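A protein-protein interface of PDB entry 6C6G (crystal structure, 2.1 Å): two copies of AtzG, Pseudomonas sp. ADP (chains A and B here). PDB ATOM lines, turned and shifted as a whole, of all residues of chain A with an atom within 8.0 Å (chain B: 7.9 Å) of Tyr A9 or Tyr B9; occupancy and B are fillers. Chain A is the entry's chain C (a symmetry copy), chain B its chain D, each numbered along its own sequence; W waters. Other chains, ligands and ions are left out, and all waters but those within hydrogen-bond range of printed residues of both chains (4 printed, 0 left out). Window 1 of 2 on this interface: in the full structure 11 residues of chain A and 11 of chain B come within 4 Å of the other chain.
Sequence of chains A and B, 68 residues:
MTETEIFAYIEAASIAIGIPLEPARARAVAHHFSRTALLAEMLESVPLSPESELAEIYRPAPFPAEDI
Ala A8 touches Ala B12, and with the chains exchanged Ala A12 touches Ala B8. Tyr A9 touches its own counterpart, Tyr B9. Tyr A9 touches Ala B12, and with the chains exchanged Ala A12 touches Tyr B9. Tyr A9 touches Ala B13, and with the chains exchanged Ala A13 touches Tyr B9. Of the 10 pairs that touch across the chains among the printed residues, 9 have their exchanged pair printed and touching as well.
OE1 of Glu B5 sits at hydrogen-bond distance from N of Thr B2, 3.1 Å away. The backbone NH (N) of Met A1 is in hydrogen-bond range of the side-chain carboxylate (OE1) of Glu A5, at 2.8 Å. The backbone NH of Glu A5 lies within hydrogen-bond range of the side-chain hydroxyl of Thr A2, 3.2 Å away.
Water W1 lies within hydrogen-bond range of O of Glu B5 (2.7 Å) and O of Ala A12 (3.0 Å). Water W2 bridges O of Glu A5 (2.8 Å) and O of Ala B12 (2.8 Å). Water W3 bridges OH of Tyr B9 (2.8 Å) and OH of Tyr A9 (3.2 Å). Water W4 bridges the side-chain hydroxyl of Tyr A9 and the side-chain hydroxyl of Tyr B9.
Of the 19 printed residues of chain A, 7 touch a printed residue of chain B. Along chain A the printed residues that touch a printed residue of chain B span positions 5 to 16. Among the printed residues, no Asp or Glu carboxylate lies within 4 Å of a Lys or Arg side-chain nitrogen of the other chain.
Of the printed residues of chain B, Glu A5 touches Ile B15. Ala A8 touches just one residue of chain B: Ala B12 (3.8 Å). Of chain B, only Tyr B9 (3.9 Å), Ala B12 (3.8 Å) and Ala B13 (3.6 Å) come within 4 Å of Tyr A9. Of the printed residues of chain B, Ala A12 touches Ala B8 (3.8 Å) and Tyr B9 (3.7 Å). Ala B8 touches just one residue of chain A: Ala A12 (3.8 Å). Printed residues of chain A within 4 Å of Tyr B9: Tyr A9, Ala A12 and Ala A13. The nearest residue of chain A that does not touch Tyr B9 is Ala A16 (4.2 Å). The nearest printed residue of chain A that does not touch Ile B15 is Met A1 (4.8 Å).
CD of Glu A5 touches CG2 of Ile B15, at 3.4 Å. CB of Ala B12 touches O of Ala A8, 3.8 Å away. CE1 of Tyr B9 touches CE1 of Tyr A9, 3.9 Å away. Tyr A9 touches Ala B12 (CA to CB, 3.8 Å). CD1 of Tyr A9 touches CA of Ala B13 (3.6 Å). CB of Ala A12 touches O of Ala B8 (3.8 Å). Ala A12 touches Tyr B9. Tyr B9 touches Ala A13 (CD1 to CA, 3.6 Å). OE2 of Glu B5 touches CG2 of Ile A15, 3.4 Å away. CE of Met B1 touches CB of Ala A16 (3.2 Å).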
ATOM      1  N   MET A   1      22.937 -18.732 -31.187  1.00  0.00           N
ATOM      2  CA  MET A   1      21.640 -19.375 -31.532  1.00  0.00           C
ATOM      3  C   MET A   1      20.792 -19.756 -30.303  1.00  0.00           C
ATOM      4  O   MET A   1      19.595 -20.007 -30.472  1.00  0.00           O
ATOM      5  CB  MET A   1      21.872 -20.572 -32.483  1.00  0.00           C
ATOM      6  N   THR A   2      21.364 -19.783 -29.093  1.00  0.00           N
ATOM      7  CA  THR A   2      20.548 -19.919 -27.887  1.00  0.00           C
ATOM      8  C   THR A   2      19.772 -18.621 -27.586  1.00  0.00           C
ATOM      9  O   THR A   2      20.127 -17.549 -28.071  1.00  0.00           O
ATOM     10  CB  THR A   2      21.370 -20.297 -26.632  1.00  0.00           C
ATOM     11  OG1 THR A   2      22.176 -19.191 -26.205  1.00  0.00           O
ATOM     12  CG2 THR A   2      22.245 -21.528 -26.886  1.00  0.00           C
ATOM     13  N   GLU A   3      18.749 -18.752 -26.743  1.00  0.00           N
ATOM     14  CA  GLU A   3      17.941 -17.653 -26.226  1.00  0.00           C
ATOM     15  C   GLU A   3      18.786 -16.557 -25.549  1.00  0.00           C
ATOM     16  O   GLU A   3      18.508 -15.351 -25.663  1.00  0.00           O
ATOM     17  CB  GLU A   3      16.988 -18.237 -25.213  1.00  0.00           C
ATOM     18  CG  GLU A   3      16.126 -17.215 -24.512  1.00  0.00           C
ATOM     19  CD  GLU A   3      14.717 -17.729 -24.319  1.00  0.00           C
ATOM     20  OE1 GLU A   3      14.227 -18.578 -25.136  1.00  0.00           O
ATOM     21  OE2 GLU A   3      14.083 -17.268 -23.333  1.00  0.00           O
ATOM     22  N   THR A   4      19.794 -16.980 -24.804  1.00  0.00           N
ATOM     23  CA  THR A   4      20.631 -15.992 -24.143  1.00  0.00           C
ATOM     24  C   THR A   4      21.598 -15.317 -25.139  1.00  0.00           C
ATOM     25  O   THR A   4      21.948 -14.165 -24.927  1.00  0.00           O
ATOM     26  CB  THR A   4      21.275 -16.513 -22.842  1.00  0.00           C
ATOM     27  OG1 THR A   4      21.055 -15.556 -21.822  1.00  0.00           O
ATOM     28  CG2 THR A   4      22.769 -16.670 -22.925  1.00  0.00           C
ATOM     29  N   GLU A   5      22.016 -16.033 -26.182  1.00  0.00           N
ATOM     30  CA  GLU A   5      22.868 -15.479 -27.212  1.00  0.00           C
ATOM     31  C   GLU A   5      22.078 -14.480 -28.059  1.00  0.00           C
ATOM     32  O   GLU A   5      22.581 -13.399 -28.364  1.00  0.00           O
ATOM     33  CB  GLU A   5      23.513 -16.582 -28.070  1.00  0.00           C
ATOM     34  CG  GLU A   5      24.641 -17.287 -27.311  1.00  0.00           C
ATOM     35  CD  GLU A   5      25.105 -18.627 -27.880  1.00  0.00           C
ATOM     36  OE1 GLU A   5      24.558 -19.139 -28.883  1.00  0.00           O
ATOM     37  OE2 GLU A   5      26.041 -19.173 -27.259  1.00  0.00           O
ATOM     38  N   ILE A   6      20.841 -14.843 -28.404  1.00  0.00           N
ATOM     39  CA  ILE A   6      19.944 -13.953 -29.146  1.00  0.00           C
ATOM     40  C   ILE A   6      19.714 -12.655 -28.366  1.00  0.00           C
ATOM     41  O   ILE A   6      19.825 -11.574 -28.917  1.00  0.00           O
ATOM     42  CB  ILE A   6      18.603 -14.627 -29.488  1.00  0.00           C
ATOM     43  CG1 ILE A   6      18.810 -15.684 -30.580  1.00  0.00           C
ATOM     44  CG2 ILE A   6      17.590 -13.616 -30.012  1.00  0.00           C
ATOM     45  CD1 ILE A   6      17.707 -16.731 -30.631  1.00  0.00           C
ATOM     46  N   PHE A   7      19.436 -12.783 -27.076  1.00  0.00           N
ATOM     47  CA  PHE A   7      19.222 -11.609 -26.241  1.00  0.00           C
ATOM     48  C   PHE A   7      20.476 -10.706 -26.159  1.00  0.00           C
ATOM     49  O   PHE A   7      20.387  -9.499 -26.308  1.00  0.00           O
ATOM     50  CB  PHE A   7      18.700 -11.999 -24.865  1.00  0.00           C
ATOM     51  CG  PHE A   7      18.191 -10.830 -24.081  1.00  0.00           C
ATOM     52  CD1 PHE A   7      17.029 -10.135 -24.501  1.00  0.00           C
ATOM     53  CD2 PHE A   7      18.849 -10.387 -22.935  1.00  0.00           C
ATOM     54  CE1 PHE A   7      16.552  -9.028 -23.778  1.00  0.00           C
ATOM     55  CE2 PHE A   7      18.354  -9.295 -22.199  1.00  0.00           C
ATOM     56  CZ  PHE A   7      17.207  -8.614 -22.624  1.00  0.00           C
ATOM     57  N   ALA A   8      21.649 -11.275 -25.958  1.00  0.00           N
ATOM     58  CA  ALA A   8      22.862 -10.464 -25.922  1.00  0.00           C
ATOM     59  C   ALA A   8      23.108  -9.756 -27.269  1.00  0.00           C
ATOM     60  O   ALA A   8      23.564  -8.623 -27.261  1.00  0.00           O
ATOM     61  CB  ALA A   8      24.088 -11.291 -25.513  1.00  0.00           C
ATOM     62  N   TYR A   9      22.768 -10.403 -28.393  1.00  0.00           N
ATOM     63  CA  TYR A   9      22.960  -9.828 -29.746  1.00  0.00           C
ATOM     64  C   TYR A   9      22.004  -8.670 -29.981  1.00  0.00           C
ATOM     65  O   TYR A   9      22.441  -7.597 -30.410  1.00  0.00           O
ATOM     66  CB  TYR A   9      22.814 -10.880 -30.882  1.00  0.00           C
ATOM     67  CG  TYR A   9      22.920 -10.229 -32.261  1.00  0.00           C
ATOM     68  CD1 TYR A   9      24.113  -9.758 -32.720  1.00  0.00           C
ATOM     69  CD2 TYR A   9      21.780 -10.024 -33.066  1.00  0.00           C
ATOM     70  CE1 TYR A   9      24.205  -9.109 -33.951  1.00  0.00           C
ATOM     71  CE2 TYR A   9      21.855  -9.408 -34.287  1.00  0.00           C
ATOM     72  CZ  TYR A   9      23.073  -8.939 -34.732  1.00  0.00           C
ATOM     73  OH  TYR A   9      23.211  -8.302 -35.963  1.00  0.00           O
ATOM     74  N   ILE A  10      20.725  -8.871 -29.671  1.00  0.00           N
ATOM     75  CA  ILE A  10      19.728  -7.799 -29.787  1.00  0.00           C
ATOM     76  C   ILE A  10      20.183  -6.559 -28.986  1.00  0.00           C
ATOM     77  O   ILE A  10      20.158  -5.436 -29.503  1.00  0.00           O
ATOM     78  CB  ILE A  10      18.295  -8.241 -29.315  1.00  0.00           C
ATOM     79  CG1 ILE A  10      17.702  -9.371 -30.161  1.00  0.00           C
ATOM     80  CG2 ILE A  10      17.322  -7.067 -29.325  1.00  0.00           C
ATOM     81  CD1 ILE A  10      17.750  -9.210 -31.650  1.00  0.00           C
ATOM     82  N   GLU A  11      20.630  -6.769 -27.745  1.00  0.00           N
ATOM     83  CA  GLU A  11      21.091  -5.649 -26.925  1.00  0.00           C
ATOM     84  C   GLU A  11      22.305  -4.945 -27.498  1.00  0.00           C
ATOM     85  O   GLU A  11      22.328  -3.730 -27.613  1.00  0.00           O
ATOM     86  CB  GLU A  11      21.363  -6.104 -25.497  1.00  0.00           C
ATOM     87  CG  GLU A  11      20.049  -6.367 -24.797  1.00  0.00           C
ATOM     88  CD  GLU A  11      20.171  -6.683 -23.313  1.00  0.00           C
ATOM     89  OE1 GLU A  11      21.150  -7.376 -22.898  1.00  0.00           O
ATOM     90  OE2 GLU A  11      19.234  -6.254 -22.584  1.00  0.00           O
ATOM     91  N   ALA A  12      23.312  -5.706 -27.892  1.00  0.00           N
ATOM     92  CA  ALA A  12      24.562  -5.094 -28.411  1.00  0.00           C
ATOM     93  C   ALA A  12      24.384  -4.457 -29.782  1.00  0.00           C
ATOM     94  O   ALA A  12      24.891  -3.360 -30.005  1.00  0.00           O
ATOM     95  CB  ALA A  12      25.723  -6.092 -28.403  1.00  0.00           C
ATOM     96  N   ALA A  13      23.678  -5.127 -30.680  1.00  0.00           N
ATOM     97  CA  ALA A  13      23.411  -4.597 -32.036  1.00  0.00           C
ATOM     98  C   ALA A  13      22.579  -3.333 -32.048  1.00  0.00           C
ATOM     99  O   ALA A  13      22.811  -2.442 -32.892  1.00  0.00           O
ATOM    100  CB  ALA A  13      22.703  -5.655 -32.901  1.00  0.00           C
ATOM    101  N   SER A  14      21.560  -3.298 -31.174  1.00  0.00           N
ATOM    102  CA  SER A  14      20.677  -2.115 -31.070  1.00  0.00           C
ATOM    103  C   SER A  14      21.473  -0.917 -30.535  1.00  0.00           C
ATOM    104  O   SER A  14      21.351   0.158 -31.079  1.00  0.00           O
ATOM    105  CB  SER A  14      19.424  -2.384 -30.224  1.00  0.00           C
ATOM    106  OG  SER A  14      19.799  -2.795 -28.916  1.00  0.00           O
ATOM    107  N   ILE A  15      22.340  -1.134 -29.544  1.00  0.00           N
ATOM    108  CA  ILE A  15      23.254  -0.061 -29.027  1.00  0.00           C
ATOM    109  C   ILE A  15      24.213   0.382 -30.127  1.00  0.00           C
ATOM    110  O   ILE A  15      24.344   1.561 -30.372  1.00  0.00           O
ATOM    111  CB  ILE A  15      23.985  -0.519 -27.732  1.00  0.00           C
ATOM    112  CG1 ILE A  15      22.986  -0.543 -26.553  1.00  0.00           C
ATOM    113  CG2 ILE A  15      25.178   0.345 -27.379  1.00  0.00           C
ATOM    114  CD1 ILE A  15      23.472  -1.391 -25.391  1.00  0.00           C
ATOM    115  N   ALA A  16      24.823  -0.546 -30.839  1.00  0.00           N
ATOM    116  CA  ALA A  16      25.704  -0.197 -31.957  1.00  0.00           C
ATOM    117  C   ALA A  16      25.104   0.721 -33.012  1.00  0.00           C
ATOM    118  O   ALA A  16      25.803   1.586 -33.525  1.00  0.00           O
ATOM    119  CB  ALA A  16      26.211  -1.454 -32.663  1.00  0.00           C
ATOM    120  N   ILE A  17      23.846   0.499 -33.377  1.00  0.00           N
ATOM    121  CA  ILE A  17      23.228   1.273 -34.442  1.00  0.00           C
ATOM    122  C   ILE A  17      22.457   2.501 -33.897  1.00  0.00           C
ATOM    123  O   ILE A  17      21.983   3.335 -34.662  1.00  0.00           O
ATOM    124  CB  ILE A  17      22.351   0.387 -35.357  1.00  0.00           C
ATOM    125  CG1 ILE A  17      22.225   0.978 -36.756  1.00  0.00           C
ATOM    126  CG2 ILE A  17      20.997   0.128 -34.740  1.00  0.00           C
ATOM    127  CD1 ILE A  17      23.535   1.023 -37.545  1.00  0.00           C
ATOM    128  N   LEU A  21      16.659   0.417 -26.468  1.00  0.00           N
ATOM    129  CA  LEU A  21      15.676  -0.608 -26.219  1.00  0.00           C
ATOM    130  C   LEU A  21      15.548  -0.872 -24.719  1.00  0.00           C
ATOM    131  O   LEU A  21      16.488  -1.374 -24.109  1.00  0.00           O
ATOM    132  CB  LEU A  21      16.054  -1.961 -26.897  1.00  0.00           C
ATOM    133  CG  LEU A  21      16.096  -2.042 -28.407  1.00  0.00           C
ATOM    134  CD1 LEU A  21      16.382  -3.479 -28.778  1.00  0.00           C
ATOM    135  CD2 LEU A  21      14.839  -1.646 -29.126  1.00  0.00           C
ATOM    136  N   PHE A  33      12.871 -11.628 -34.194  1.00  0.00           N
ATOM    137  CA  PHE A  33      14.196 -11.971 -34.736  1.00  0.00           C
ATOM    138  C   PHE A  33      14.406 -13.472 -34.822  1.00  0.00           C
ATOM    139  O   PHE A  33      14.931 -13.979 -35.821  1.00  0.00           O
ATOM    140  CB  PHE A  33      15.293 -11.354 -33.869  1.00  0.00           C
ATOM    141  CG  PHE A  33      16.679 -11.556 -34.389  1.00  0.00           C
ATOM    142  CD1 PHE A  33      17.399 -12.713 -34.062  1.00  0.00           C
ATOM    143  CD2 PHE A  33      17.270 -10.613 -35.207  1.00  0.00           C
ATOM    144  CE1 PHE A  33      18.689 -12.910 -34.559  1.00  0.00           C
ATOM    145  CE2 PHE A  33      18.558 -10.784 -35.686  1.00  0.00           C
ATOM    146  CZ  PHE A  33      19.286 -11.923 -35.364  1.00  0.00           C
ATOM    147  N   MET B   1      30.294   4.709 -31.481  1.00  0.00           N
ATOM    148  CA  MET B   1      30.224   3.758 -30.339  1.00  0.00           C
ATOM    149  C   MET B   1      31.542   3.733 -29.585  1.00  0.00           C
ATOM    150  O   MET B   1      32.614   3.782 -30.197  1.00  0.00           O
ATOM    151  CB  MET B   1      29.878   2.340 -30.822  1.00  0.00           C
ATOM    152  CG  MET B   1      30.272   1.919 -32.268  1.00  0.00           C
ATOM    153  SD  MET B   1      29.473   0.380 -32.913  1.00  0.00           S
ATOM    154  CE  MET B   1      29.009  -0.458 -31.351  1.00  0.00           C
ATOM    155  N   THR B   2      31.449   3.580 -28.275  1.00  0.00           N
ATOM    156  CA  THR B   2      32.607   3.439 -27.398  1.00  0.00           C
ATOM    157  C   THR B   2      33.296   2.070 -27.621  1.00  0.00           C
ATOM    158  O   THR B   2      32.716   1.115 -28.180  1.00  0.00           O
ATOM    159  CB  THR B   2      32.201   3.527 -25.902  1.00  0.00           C
ATOM    160  OG1 THR B   2      31.404   2.391 -25.514  1.00  0.00           O
ATOM    161  CG2 THR B   2      31.390   4.783 -25.595  1.00  0.00           C
ATOM    162  N   GLU B   3      34.531   1.998 -27.151  1.00  0.00           N
ATOM    163  CA  GLU B   3      35.347   0.781 -27.162  1.00  0.00           C
ATOM    164  C   GLU B   3      34.672  -0.376 -26.411  1.00  0.00           C
ATOM    165  O   GLU B   3      34.779  -1.541 -26.817  1.00  0.00           O
ATOM    166  CB  GLU B   3      36.700   1.120 -26.563  1.00  0.00           C
ATOM    167  CG  GLU B   3      37.667  -0.041 -26.475  1.00  0.00           C
ATOM    168  CD  GLU B   3      39.113   0.374 -26.068  1.00  0.00           C
ATOM    169  OE1 GLU B   3      39.275   1.035 -24.996  1.00  0.00           O
ATOM    170  OE2 GLU B   3      40.072   0.006 -26.808  1.00  0.00           O
ATOM    171  N   THR B   4      33.956  -0.066 -25.328  1.00  0.00           N
ATOM    172  CA  THR B   4      33.199  -1.077 -24.613  1.00  0.00           C
ATOM    173  C   THR B   4      32.010  -1.606 -25.389  1.00  0.00           C
ATOM    174  O   THR B   4      31.686  -2.798 -25.323  1.00  0.00           O
ATOM    175  CB  THR B   4      32.681  -0.487 -23.308  1.00  0.00           C
ATOM    176  OG1 THR B   4      33.809  -0.189 -22.487  1.00  0.00           O
ATOM    177  CG2 THR B   4      31.753  -1.445 -22.554  1.00  0.00           C
ATOM    178  N   GLU B   5      31.345  -0.699 -26.106  1.00  0.00           N
ATOM    179  CA  GLU B   5      30.177  -1.049 -26.920  1.00  0.00           C
ATOM    180  C   GLU B   5      30.613  -1.884 -28.114  1.00  0.00           C
ATOM    181  O   GLU B   5      29.953  -2.892 -28.415  1.00  0.00           O
ATOM    182  CB  GLU B   5      29.414   0.213 -27.382  1.00  0.00           C
ATOM    183  CG  GLU B   5      28.596   0.828 -26.242  1.00  0.00           C
ATOM    184  CD  GLU B   5      28.070   2.234 -26.532  1.00  0.00           C
ATOM    185  OE1 GLU B   5      28.510   2.936 -27.484  1.00  0.00           O
ATOM    186  OE2 GLU B   5      27.165   2.635 -25.790  1.00  0.00           O
ATOM    187  N   ILE B   6      31.727  -1.471 -28.752  1.00  0.00           N
ATOM    188  CA  ILE B   6      32.303  -2.239 -29.846  1.00  0.00           C
ATOM    189  C   ILE B   6      32.665  -3.651 -29.396  1.00  0.00           C
ATOM    190  O   ILE B   6      32.327  -4.609 -30.070  1.00  0.00           O
ATOM    191  CB  ILE B   6      33.522  -1.545 -30.475  1.00  0.00           C
ATOM    192  CG1 ILE B   6      33.080  -0.296 -31.253  1.00  0.00           C
ATOM    193  CG2 ILE B   6      34.212  -2.495 -31.472  1.00  0.00           C
ATOM    194  CD1 ILE B   6      34.230   0.639 -31.578  1.00  0.00           C
ATOM    195  N   PHE B   7      33.311  -3.779 -28.243  1.00  0.00           N
ATOM    196  CA  PHE B   7      33.680  -5.102 -27.677  1.00  0.00           C
ATOM    197  C   PHE B   7      32.431  -5.973 -27.469  1.00  0.00           C
ATOM    198  O   PHE B   7      32.419  -7.121 -27.892  1.00  0.00           O
ATOM    199  CB  PHE B   7      34.501  -4.939 -26.372  1.00  0.00           C
ATOM    200  CG  PHE B   7      34.865  -6.244 -25.681  1.00  0.00           C
ATOM    201  CD1 PHE B   7      33.898  -6.952 -24.901  1.00  0.00           C
ATOM    202  CD2 PHE B   7      36.149  -6.781 -25.772  1.00  0.00           C
ATOM    203  CE1 PHE B   7      34.218  -8.154 -24.278  1.00  0.00           C
ATOM    204  CE2 PHE B   7      36.476  -7.994 -25.152  1.00  0.00           C
ATOM    205  CZ  PHE B   7      35.527  -8.689 -24.403  1.00  0.00           C
ATOM    206  N   ALA B   8      31.401  -5.445 -26.819  1.00  0.00           N
ATOM    207  CA  ALA B   8      30.207  -6.255 -26.571  1.00  0.00           C
ATOM    208  C   ALA B   8      29.547  -6.707 -27.897  1.00  0.00           C
ATOM    209  O   ALA B   8      29.076  -7.845 -27.989  1.00  0.00           O
ATOM    210  CB  ALA B   8      29.227  -5.533 -25.674  1.00  0.00           C
ATOM    211  N   TYR B   9      29.588  -5.838 -28.914  1.00  0.00           N
ATOM    212  CA  TYR B   9      28.963  -6.116 -30.213  1.00  0.00           C
ATOM    213  C   TYR B   9      29.726  -7.188 -30.978  1.00  0.00           C
ATOM    214  O   TYR B   9      29.126  -8.150 -31.456  1.00  0.00           O
ATOM    215  CB  TYR B   9      28.815  -4.846 -31.097  1.00  0.00           C
ATOM    216  CG  TYR B   9      28.203  -5.171 -32.445  1.00  0.00           C
ATOM    217  CD1 TYR B   9      26.865  -5.552 -32.547  1.00  0.00           C
ATOM    218  CD2 TYR B   9      28.987  -5.201 -33.608  1.00  0.00           C
ATOM    219  CE1 TYR B   9      26.309  -5.876 -33.790  1.00  0.00           C
ATOM    220  CE2 TYR B   9      28.433  -5.524 -34.831  1.00  0.00           C
ATOM    221  CZ  TYR B   9      27.096  -5.862 -34.920  1.00  0.00           C
ATOM    222  OH  TYR B   9      26.559  -6.176 -36.148  1.00  0.00           O
ATOM    223  N   ILE B  10      31.047  -7.030 -31.073  1.00  0.00           N
ATOM    224  CA  ILE B  10      31.911  -8.034 -31.722  1.00  0.00           C
ATOM    225  C   ILE B  10      31.680  -9.392 -31.073  1.00  0.00           C
ATOM    226  O   ILE B  10      31.482 -10.381 -31.786  1.00  0.00           O
ATOM    227  CB  ILE B  10      33.417  -7.656 -31.691  1.00  0.00           C
ATOM    228  CG1 ILE B  10      33.695  -6.385 -32.530  1.00  0.00           C
ATOM    229  CG2 ILE B  10      34.318  -8.793 -32.231  1.00  0.00           C
ATOM    230  CD1 ILE B  10      33.162  -6.360 -33.946  1.00  0.00           C
ATOM    231  N   GLU B  11      31.648  -9.461 -29.744  1.00  0.00           N
ATOM    232  CA  GLU B  11      31.450 -10.755 -29.080  1.00  0.00           C
ATOM    233  C   GLU B  11      30.083 -11.362 -29.411  1.00  0.00           C
ATOM    234  O   GLU B  11      29.999 -12.545 -29.792  1.00  0.00           O
ATOM    235  CB  GLU B  11      31.609 -10.628 -27.569  1.00  0.00           C
ATOM    236  CG  GLU B  11      31.536 -11.968 -26.790  1.00  0.00           C
ATOM    237  CD  GLU B  11      31.842 -11.750 -25.317  1.00  0.00           C
ATOM    238  OE1 GLU B  11      33.040 -11.510 -24.968  1.00  0.00           O
ATOM    239  OE2 GLU B  11      30.871 -11.746 -24.511  1.00  0.00           O
ATOM    240  N   ALA B  12      29.011 -10.576 -29.253  1.00  0.00           N
ATOM    241  CA  ALA B  12      27.666 -11.116 -29.437  1.00  0.00           C
ATOM    242  C   ALA B  12      27.357 -11.443 -30.915  1.00  0.00           C
ATOM    243  O   ALA B  12      26.778 -12.487 -31.204  1.00  0.00           O
ATOM    244  CB  ALA B  12      26.606 -10.185 -28.867  1.00  0.00           C
ATOM    245  N   ALA B  13      27.758 -10.545 -31.820  1.00  0.00           N
ATOM    246  CA  ALA B  13      27.520 -10.731 -33.254  1.00  0.00           C
ATOM    247  C   ALA B  13      28.275 -11.899 -33.847  1.00  0.00           C
ATOM    248  O   ALA B  13      27.745 -12.576 -34.731  1.00  0.00           O
ATOM    249  CB  ALA B  13      27.867  -9.462 -34.043  1.00  0.00           C
ATOM    250  N   SER B  14      29.524 -12.087 -33.404  1.00  0.00           N
ATOM    251  CA  SER B  14      30.365 -13.190 -33.894  1.00  0.00           C
ATOM    252  C   SER B  14      29.771 -14.539 -33.429  1.00  0.00           C
ATOM    253  O   SER B  14      29.661 -15.457 -34.237  1.00  0.00           O
ATOM    254  CB  SER B  14      31.832 -13.050 -33.474  1.00  0.00           C
ATOM    255  OG  SER B  14      31.957 -13.024 -32.028  1.00  0.00           O
ATOM    256  N   ILE B  15      29.297 -14.603 -32.172  1.00  0.00           N
ATOM    257  CA  ILE B  15      28.584 -15.814 -31.663  1.00  0.00           C
ATOM    258  C   ILE B  15      27.308 -16.060 -32.472  1.00  0.00           C
ATOM    259  O   ILE B  15      27.098 -17.159 -32.960  1.00  0.00           O
ATOM    260  CB  ILE B  15      28.324 -15.729 -30.136  1.00  0.00           C
ATOM    261  CG1 ILE B  15      29.631 -15.925 -29.360  1.00  0.00           C
ATOM    262  CG2 ILE B  15      27.374 -16.811 -29.667  1.00  0.00           C
ATOM    263  CD1 ILE B  15      29.553 -15.405 -27.928  1.00  0.00           C
ATOM    264  N   ALA B  16      26.506 -15.024 -32.677  1.00  0.00           N
ATOM    265  CA  ALA B  16      25.274 -15.160 -33.465  1.00  0.00           C
ATOM    266  C   ALA B  16      25.448 -15.717 -34.861  1.00  0.00           C
ATOM    267  O   ALA B  16      24.617 -16.491 -35.320  1.00  0.00           O
ATOM    268  CB  ALA B  16      24.583 -13.819 -33.584  1.00  0.00           C
ATOM    269  N   ILE B  17      26.504 -15.313 -35.564  1.00  0.00           N
ATOM    270  CA  ILE B  17      26.699 -15.707 -36.958  1.00  0.00           C
ATOM    271  C   ILE B  17      27.556 -16.970 -37.073  1.00  0.00           C
ATOM    272  O   ILE B  17      27.742 -17.496 -38.179  1.00  0.00           O
ATOM    273  CB  ILE B  17      27.306 -14.528 -37.757  1.00  0.00           C
ATOM    274  CG1 ILE B  17      27.014 -14.604 -39.235  1.00  0.00           C
ATOM    275  CG2 ILE B  17      28.821 -14.414 -37.597  1.00  0.00           C
ATOM    276  CD1 ILE B  17      25.536 -14.408 -39.565  1.00  0.00           C
ATOM    277  N   LEU B  21      35.113 -16.224 -31.455  1.00  0.00           N
ATOM    278  CA  LEU B  21      36.405 -15.533 -31.462  1.00  0.00           C
ATOM    279  C   LEU B  21      37.113 -15.639 -30.123  1.00  0.00           C
ATOM    280  O   LEU B  21      36.587 -15.196 -29.124  1.00  0.00           O
ATOM    281  CB  LEU B  21      36.226 -14.072 -31.865  1.00  0.00           C
ATOM    282  CG  LEU B  21      35.596 -13.792 -33.251  1.00  0.00           C
ATOM    283  CD1 LEU B  21      35.305 -12.324 -33.431  1.00  0.00           C
ATOM    284  CD2 LEU B  21      36.483 -14.325 -34.405  1.00  0.00           C
ATOM    285  N   PHE B  33      37.088  -3.186 -37.136  1.00  0.00           N
ATOM    286  CA  PHE B  33      35.698  -2.735 -37.087  1.00  0.00           C
ATOM    287  C   PHE B  33      35.553  -1.262 -36.700  1.00  0.00           C
ATOM    288  O   PHE B  33      34.758  -0.513 -37.306  1.00  0.00           O
ATOM    289  CB  PHE B  33      34.916  -3.579 -36.102  1.00  0.00           C
ATOM    290  CG  PHE B  33      33.447  -3.304 -36.089  1.00  0.00           C
ATOM    291  CD1 PHE B  33      32.585  -3.977 -36.952  1.00  0.00           C
ATOM    292  CD2 PHE B  33      32.915  -2.396 -35.180  1.00  0.00           C
ATOM    293  CE1 PHE B  33      31.211  -3.738 -36.906  1.00  0.00           C
ATOM    294  CE2 PHE B  33      31.552  -2.143 -35.140  1.00  0.00           C
ATOM    295  CZ  PHE B  33      30.693  -2.807 -36.019  1.00  0.00           C
HETATM  296  O   HOH W   1      27.288  -2.680 -28.391  1.00  0.00           O
HETATM  297  O   HOH W   2      25.287 -13.627 -29.068  1.00  0.00           O
HETATM  298  O   HOH W   3      23.899  -5.256 -36.472  1.00  0.00           O
HETATM  299  O   HOH W   4      25.591  -9.082 -37.411  1.00  0.00           O
